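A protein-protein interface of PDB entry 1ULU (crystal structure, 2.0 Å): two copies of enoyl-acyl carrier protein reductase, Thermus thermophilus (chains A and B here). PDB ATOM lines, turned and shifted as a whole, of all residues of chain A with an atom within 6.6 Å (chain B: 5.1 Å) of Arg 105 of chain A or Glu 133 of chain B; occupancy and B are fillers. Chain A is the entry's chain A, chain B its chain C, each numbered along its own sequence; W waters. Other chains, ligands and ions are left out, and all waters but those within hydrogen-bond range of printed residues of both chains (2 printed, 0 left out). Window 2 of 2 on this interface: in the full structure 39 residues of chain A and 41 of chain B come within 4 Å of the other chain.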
ATOM      1  N   GLU A 100      32.522  -9.270   7.911  1.00  0.00           N
ATOM      2  CA  GLU A 100      31.147  -8.783   7.901  1.00  0.00           C
ATOM      3  C   GLU A 100      30.958  -7.619   8.869  1.00  0.00           C
ATOM      4  O   GLU A 100      30.282  -6.640   8.555  1.00  0.00           O
ATOM      5  CB  GLU A 100      30.190  -9.915   8.283  1.00  0.00           C
ATOM      6  CG  GLU A 100      30.133 -11.066   7.288  1.00  0.00           C
ATOM      7  CD  GLU A 100      29.245 -10.769   6.092  1.00  0.00           C
ATOM      8  OE1 GLU A 100      29.096 -11.659   5.226  1.00  0.00           O
ATOM      9  OE2 GLU A 100      28.693  -9.647   6.018  1.00  0.00           O
ATOM     10  N   ALA A 101      31.554  -7.737  10.051  1.00  0.00           N
ATOM     11  CA  ALA A 101      31.442  -6.702  11.065  1.00  0.00           C
ATOM     12  C   ALA A 101      32.204  -5.443  10.677  1.00  0.00           C
ATOM     13  O   ALA A 101      31.767  -4.335  10.975  1.00  0.00           O
ATOM     14  CB  ALA A 101      31.947  -7.227  12.402  1.00  0.00           C
ATOM     15  N   MET A 102      33.340  -5.612  10.008  1.00  0.00           N
ATOM     16  CA  MET A 102      34.158  -4.475   9.608  1.00  0.00           C
ATOM     17  C   MET A 102      33.638  -3.726   8.391  1.00  0.00           C
ATOM     18  O   MET A 102      34.073  -2.610   8.109  1.00  0.00           O
ATOM     19  CB  MET A 102      35.603  -4.926   9.387  1.00  0.00           C
ATOM     20  CG  MET A 102      36.262  -5.432  10.665  1.00  0.00           C
ATOM     21  SD  MET A 102      36.077  -4.158  12.136  1.00  0.00           S
ATOM     22  CE  MET A 102      34.365  -4.722  12.801  1.00  0.00           C
ATOM     23  N   GLU A 103      32.708  -4.336   7.668  1.00  0.00           N
ATOM     24  CA  GLU A 103      32.119  -3.684   6.506  1.00  0.00           C
ATOM     25  C   GLU A 103      30.749  -3.161   6.924  1.00  0.00           C
ATOM     26  O   GLU A 103      29.952  -3.889   7.516  1.00  0.00           O
ATOM     27  CB  GLU A 103      31.981  -4.670   5.338  1.00  0.00           C
ATOM     28  CG  GLU A 103      31.178  -5.930   5.645  1.00  0.00           C
ATOM     29  CD  GLU A 103      30.998  -6.823   4.423  1.00  0.00           C
ATOM     30  OE1 GLU A 103      30.315  -6.396   3.467  1.00  0.00           O
ATOM     31  OE2 GLU A 103      31.542  -7.950   4.415  1.00  0.00           O
ATOM     32  N   GLY A 104      30.482  -1.895   6.635  1.00  0.00           N
ATOM     33  CA  GLY A 104      29.199  -1.327   7.002  1.00  0.00           C
ATOM     34  C   GLY A 104      29.253  -0.494   8.269  1.00  0.00           C
ATOM     35  O   GLY A 104      30.281   0.102   8.588  1.00  0.00           O
ATOM     36  N   ARG A 105      28.145  -0.470   9.001  1.00  0.00           N
ATOM     37  CA  ARG A 105      28.053   0.316  10.221  1.00  0.00           C
ATOM     38  C   ARG A 105      28.150  -0.520  11.492  1.00  0.00           C
ATOM     39  O   ARG A 105      27.790  -1.697  11.516  1.00  0.00           O
ATOM     40  CB  ARG A 105      26.735   1.097  10.233  1.00  0.00           C
ATOM     41  CG  ARG A 105      26.449   1.870   8.954  1.00  0.00           C
ATOM     42  CD  ARG A 105      25.189   2.698   9.102  1.00  0.00           C
ATOM     43  NE  ARG A 105      24.033   1.877   9.446  1.00  0.00           N
ATOM     44  CZ  ARG A 105      22.902   2.364   9.948  1.00  0.00           C
ATOM     45  NH1 ARG A 105      22.781   3.667  10.164  1.00  0.00           N
ATOM     46  NH2 ARG A 105      21.899   1.550  10.246  1.00  0.00           N
ATOM     47  N   TYR A 106      28.638   0.105  12.554  1.00  0.00           N
ATOM     48  CA  TYR A 106      28.766  -0.580  13.826  1.00  0.00           C
ATOM     49  C   TYR A 106      27.384  -1.003  14.315  1.00  0.00           C
ATOM     50  O   TYR A 106      27.199  -2.115  14.806  1.00  0.00           O
ATOM     51  CB  TYR A 106      29.424   0.338  14.866  1.00  0.00           C
ATOM     52  CG  TYR A 106      29.449  -0.275  16.247  1.00  0.00           C
ATOM     53  CD1 TYR A 106      30.075  -1.503  16.468  1.00  0.00           C
ATOM     54  CD2 TYR A 106      28.809   0.342  17.320  1.00  0.00           C
ATOM     55  CE1 TYR A 106      30.057  -2.104  17.717  1.00  0.00           C
ATOM     56  CE2 TYR A 106      28.785  -0.254  18.585  1.00  0.00           C
ATOM     57  CZ  TYR A 106      29.412  -1.481  18.771  1.00  0.00           C
ATOM     58  OH  TYR A 106      29.381  -2.100  19.996  1.00  0.00           O
ATOM     59  N   ILE A 107      26.412  -0.113  14.158  1.00  0.00           N
ATOM     60  CA  ILE A 107      25.055  -0.390  14.603  1.00  0.00           C
ATOM     61  C   ILE A 107      24.453  -1.612  13.905  1.00  0.00           C
ATOM     62  O   ILE A 107      23.508  -2.216  14.411  1.00  0.00           O
ATOM     63  CB  ILE A 107      24.139   0.864  14.408  1.00  0.00           C
ATOM     64  CG1 ILE A 107      22.728   0.578  14.921  1.00  0.00           C
ATOM     65  CG2 ILE A 107      24.068   1.258  12.944  1.00  0.00           C
ATOM     66  CD1 ILE A 107      22.678   0.117  16.341  1.00  0.00           C
ATOM     67  N   ASP A 108      25.015  -1.998  12.764  1.00  0.00           N
ATOM     68  CA  ASP A 108      24.498  -3.155  12.038  1.00  0.00           C
ATOM     69  C   ASP A 108      25.248  -4.451  12.316  1.00  0.00           C
ATOM     70  O   ASP A 108      25.002  -5.465  11.662  1.00  0.00           O
ATOM     71  CB  ASP A 108      24.505  -2.892  10.526  1.00  0.00           C
ATOM     72  CG  ASP A 108      23.532  -1.808  10.121  1.00  0.00           C
ATOM     73  OD1 ASP A 108      22.449  -1.723  10.741  1.00  0.00           O
ATOM     74  OD2 ASP A 108      23.840  -1.047   9.181  1.00  0.00           O
ATOM     75  N   THR A 109      26.147  -4.427  13.294  1.00  0.00           N
ATOM     76  CA  THR A 109      26.932  -5.610  13.620  1.00  0.00           C
ATOM     77  C   THR A 109      26.069  -6.785  14.070  1.00  0.00           C
ATOM     78  O   THR A 109      25.240  -6.652  14.974  1.00  0.00           O
ATOM     79  CB  THR A 109      27.961  -5.317  14.734  1.00  0.00           C
ATOM     80  OG1 THR A 109      28.737  -4.164  14.381  1.00  0.00           O
ATOM     81  CG2 THR A 109      28.892  -6.510  14.914  1.00  0.00           C
ATOM     82  N   ASN A 158      34.581   0.224  13.610  1.00  0.00           N
ATOM     83  CA  ASN A 158      33.472  -0.532  14.188  1.00  0.00           C
ATOM     84  C   ASN A 158      33.743  -1.327  15.468  1.00  0.00           C
ATOM     85  O   ASN A 158      34.301  -0.795  16.425  1.00  0.00           O
ATOM     86  CB  ASN A 158      32.889  -1.453  13.113  1.00  0.00           C
ATOM     87  CG  ASN A 158      32.363  -0.685  11.909  1.00  0.00           C
ATOM     88  OD1 ASN A 158      31.928  -1.276  10.919  1.00  0.00           O
ATOM     89  ND2 ASN A 158      32.394   0.637  11.992  1.00  0.00           N
ATOM     90  N   VAL B 128      19.264  -3.219  20.140  1.00  0.00           N
ATOM     91  CA  VAL B 128      18.046  -2.422  20.234  1.00  0.00           C
ATOM     92  C   VAL B 128      18.165  -1.102  19.484  1.00  0.00           C
ATOM     93  O   VAL B 128      17.186  -0.613  18.914  1.00  0.00           O
ATOM     94  CB  VAL B 128      17.656  -2.171  21.701  1.00  0.00           C
ATOM     95  CG1 VAL B 128      17.472  -3.502  22.399  1.00  0.00           C
ATOM     96  CG2 VAL B 128      18.719  -1.340  22.414  1.00  0.00           C
ATOM     97  N   ALA B 129      19.366  -0.534  19.463  1.00  0.00           N
ATOM     98  CA  ALA B 129      19.584   0.713  18.753  1.00  0.00           C
ATOM     99  C   ALA B 129      19.315   0.497  17.265  1.00  0.00           C
ATOM    100  O   ALA B 129      18.712   1.341  16.603  1.00  0.00           O
ATOM    101  CB  ALA B 129      21.014   1.196  18.964  1.00  0.00           C
ATOM    102  N   ARG B 130      19.747  -0.642  16.736  1.00  0.00           N
ATOM    103  CA  ARG B 130      19.535  -0.905  15.323  1.00  0.00           C
ATOM    104  C   ARG B 130      18.052  -1.021  14.998  1.00  0.00           C
ATOM    105  O   ARG B 130      17.592  -0.530  13.970  1.00  0.00           O
ATOM    106  CB  ARG B 130      20.232  -2.191  14.892  1.00  0.00           C
ATOM    107  CG  ARG B 130      20.298  -2.330  13.384  1.00  0.00           C
ATOM    108  CD  ARG B 130      20.637  -3.736  12.968  1.00  0.00           C
ATOM    109  NE  ARG B 130      19.493  -4.627  13.117  1.00  0.00           N
ATOM    110  CZ  ARG B 130      19.570  -5.846  13.636  1.00  0.00           C
ATOM    111  NH1 ARG B 130      20.742  -6.310  14.059  1.00  0.00           N
ATOM    112  NH2 ARG B 130      18.484  -6.603  13.724  1.00  0.00           N
ATOM    113  N   ARG B 131      17.306  -1.674  15.879  1.00  0.00           N
ATOM    114  CA  ARG B 131      15.881  -1.860  15.663  1.00  0.00           C
ATOM    115  C   ARG B 131      15.084  -0.596  15.946  1.00  0.00           C
ATOM    116  O   ARG B 131      14.023  -0.379  15.365  1.00  0.00           O
ATOM    117  CB  ARG B 131      15.376  -3.022  16.524  1.00  0.00           C
ATOM    118  CG  ARG B 131      16.009  -4.355  16.143  1.00  0.00           C
ATOM    119  CD  ARG B 131      15.570  -5.477  17.065  1.00  0.00           C
ATOM    120  NE  ARG B 131      15.980  -6.789  16.570  1.00  0.00           N
ATOM    121  CZ  ARG B 131      17.231  -7.246  16.561  1.00  0.00           C
ATOM    122  NH1 ARG B 131      18.227  -6.500  17.027  1.00  0.00           N
ATOM    123  NH2 ARG B 131      17.483  -8.457  16.083  1.00  0.00           N
ATOM    124  N   ALA B 132      15.597   0.250  16.832  1.00  0.00           N
ATOM    125  CA  ALA B 132      14.901   1.487  17.155  1.00  0.00           C
ATOM    126  C   ALA B 132      15.137   2.554  16.088  1.00  0.00           C
ATOM    127  O   ALA B 132      14.291   3.420  15.875  1.00  0.00           O
ATOM    128  CB  ALA B 132      15.357   2.006  18.524  1.00  0.00           C
ATOM    129  N   GLU B 133      16.279   2.483  15.408  1.00  0.00           N
ATOM    130  CA  GLU B 133      16.615   3.478  14.398  1.00  0.00           C
ATOM    131  C   GLU B 133      15.463   3.843  13.455  1.00  0.00           C
ATOM    132  O   GLU B 133      15.139   5.020  13.297  1.00  0.00           O
ATOM    133  CB  GLU B 133      17.836   3.029  13.587  1.00  0.00           C
ATOM    134  CG  GLU B 133      18.256   4.023  12.510  1.00  0.00           C
ATOM    135  CD  GLU B 133      19.564   3.645  11.842  1.00  0.00           C
ATOM    136  OE1 GLU B 133      19.923   2.451  11.867  1.00  0.00           O
ATOM    137  OE2 GLU B 133      20.228   4.541  11.279  1.00  0.00           O
ATOM    138  N   PRO B 134      14.823   2.842  12.831  1.00  0.00           N
ATOM    139  CA  PRO B 134      13.710   3.102  11.909  1.00  0.00           C
ATOM    140  C   PRO B 134      12.503   3.742  12.596  1.00  0.00           C
ATOM    141  O   PRO B 134      11.776   4.533  11.993  1.00  0.00           O
ATOM    142  CB  PRO B 134      13.362   1.709  11.372  1.00  0.00           C
ATOM    143  CG  PRO B 134      14.592   0.904  11.610  1.00  0.00           C
ATOM    144  CD  PRO B 134      15.075   1.396  12.938  1.00  0.00           C
ATOM    145  N   LEU B 135      12.284   3.388  13.857  1.00  0.00           N
ATOM    146  CA  LEU B 135      11.147   3.915  14.600  1.00  0.00           C
ATOM    147  C   LEU B 135      11.364   5.291  15.216  1.00  0.00           C
ATOM    148  O   LEU B 135      10.421   6.070  15.342  1.00  0.00           O
ATOM    149  CB  LEU B 135      10.748   2.944  15.711  1.00  0.00           C
ATOM    150  CG  LEU B 135      10.408   1.511  15.310  1.00  0.00           C
ATOM    151  CD1 LEU B 135       9.913   0.767  16.538  1.00  0.00           C
ATOM    152  CD2 LEU B 135       9.345   1.508  14.221  1.00  0.00           C
ATOM    153  N   LEU B 136      12.600   5.583  15.612  1.00  0.00           N
ATOM    154  CA  LEU B 136      12.917   6.856  16.252  1.00  0.00           C
ATOM    155  C   LEU B 136      12.669   8.097  15.397  1.00  0.00           C
ATOM    156  O   LEU B 136      13.130   8.195  14.260  1.00  0.00           O
ATOM    157  CB  LEU B 136      14.366   6.837  16.743  1.00  0.00           C
ATOM    158  CG  LEU B 136      14.613   5.877  17.911  1.00  0.00           C
ATOM    159  CD1 LEU B 136      16.101   5.697  18.139  1.00  0.00           C
ATOM    160  CD2 LEU B 136      13.931   6.421  19.157  1.00  0.00           C
ATOM    161  N   GLU B 177      26.793   7.316  14.288  1.00  0.00           N
ATOM    162  CA  GLU B 177      25.985   6.719  13.228  1.00  0.00           C
ATOM    163  C   GLU B 177      24.511   7.112  13.206  1.00  0.00           C
ATOM    164  O   GLU B 177      23.881   7.081  12.153  1.00  0.00           O
ATOM    165  CB  GLU B 177      26.114   5.192  13.272  1.00  0.00           C
ATOM    166  CG  GLU B 177      27.562   4.719  13.287  1.00  0.00           C
ATOM    167  CD  GLU B 177      27.720   3.229  13.060  1.00  0.00           C
ATOM    168  OE1 GLU B 177      26.905   2.440  13.585  1.00  0.00           O
ATOM    169  OE2 GLU B 177      28.678   2.843  12.364  1.00  0.00           O
ATOM    170  N   LEU B 178      23.958   7.492  14.351  1.00  0.00           N
ATOM    171  CA  LEU B 178      22.552   7.863  14.403  1.00  0.00           C
ATOM    172  C   LEU B 178      22.326   9.369  14.469  1.00  0.00           C
ATOM    173  O   LEU B 178      21.199   9.840  14.305  1.00  0.00           O
ATOM    174  CB  LEU B 178      21.886   7.191  15.603  1.00  0.00           C
ATOM    175  CG  LEU B 178      22.047   5.669  15.674  1.00  0.00           C
ATOM    176  CD1 LEU B 178      21.295   5.137  16.877  1.00  0.00           C
ATOM    177  CD2 LEU B 178      21.523   5.033  14.399  1.00  0.00           C
HETATM  178  O   HOH W   1      22.980  -4.889  15.161  1.00  0.00           O
HETATM  179  O   HOH W   2      24.600   5.858   9.758  1.00  0.00           O
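OE1 of Glu 133 of chain B lies within salt-bridge range of NH2 of Arg 105 of chain A (2.7 Å).
The backbone NH (N) of Ile 107 of chain A lies within hydrogen-bond range of the side-chain carboxylate (OE1) of Glu 177 of chain B (2.7 Å).
N of Tyr 106 of chain A lies within hydrogen-bond range of OE2 of Glu 177 of chain B (2.7 Å).
Arg 105 of chain A touches two residues of chain B.
Of chain A, only Arg 105 comes within 4 Å of Glu 133 of chain B.
Of the printed residues of chain B, Asp 108 of chain A touches Arg 130 (3.5 Å).
Of the printed residues of chain B, Ile 107 of chain A touches Ala 129 (3.3 Å), Arg 130 (3.1 Å) and Glu 177 (2.7 Å).
Gly 104 of chain A touches none of the printed residues of chain B.
Met 102 of chain A touches none of the printed residues of chain B.
The nearest residue of chain B that does not touch Arg 105 of chain A is Leu 178 of chain B (4.6 Å).
The nearest residue of chain A that does not touch Glu 133 of chain B is Ile 107 of chain A (4.4 Å).
No position is printed for both chains.
Printed residues of chain A that touch a printed residue of chain B: Arg 105, Tyr 106, Ile 107 and Asp 108.
Among the printed residues, 7 pairs touch across the chains.
Among the printed residues, Asp or Glu carboxylates within 4 Å of a Lys or Arg side-chain nitrogen of the other chain: Arg 105 of chain A with Glu 133 of chain B (2.7 Å).
The side-chain carboxylate (OD2) of Asp 108 of chain A is in salt-bridge range of the guanidinium group (NE) of Arg 105 of chain A (2.9 Å).
The backbone carbonyl oxygen (O) of Tyr 106 of chain A is in hydrogen-bond range of the side-chain hydroxyl (OG1) of Thr 109 of chain A (2.6 Å).
Water W2 bridges the backbone carbonyl oxygen (O) of Glu 177 of chain B and the guanidinium group (NH1) of Arg 105 of chain A.
Water W1 lies within hydrogen-bond range of O of Ile 107 of chain A (2.8 Å), NH1 of Arg 130 of chain B (2.9 Å) and O of Thr 109 of chain A (2.9 Å).
Among the printed residues, pairs that only touch across the chains: Arg 105 of chain A with Glu 177 of chain B, Ile 107 of chain A with Ala 129 of chain B, Ile 107 of chain A with Arg 130 of chain B and Asp 108 of chain A with Arg 130 of chain B.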
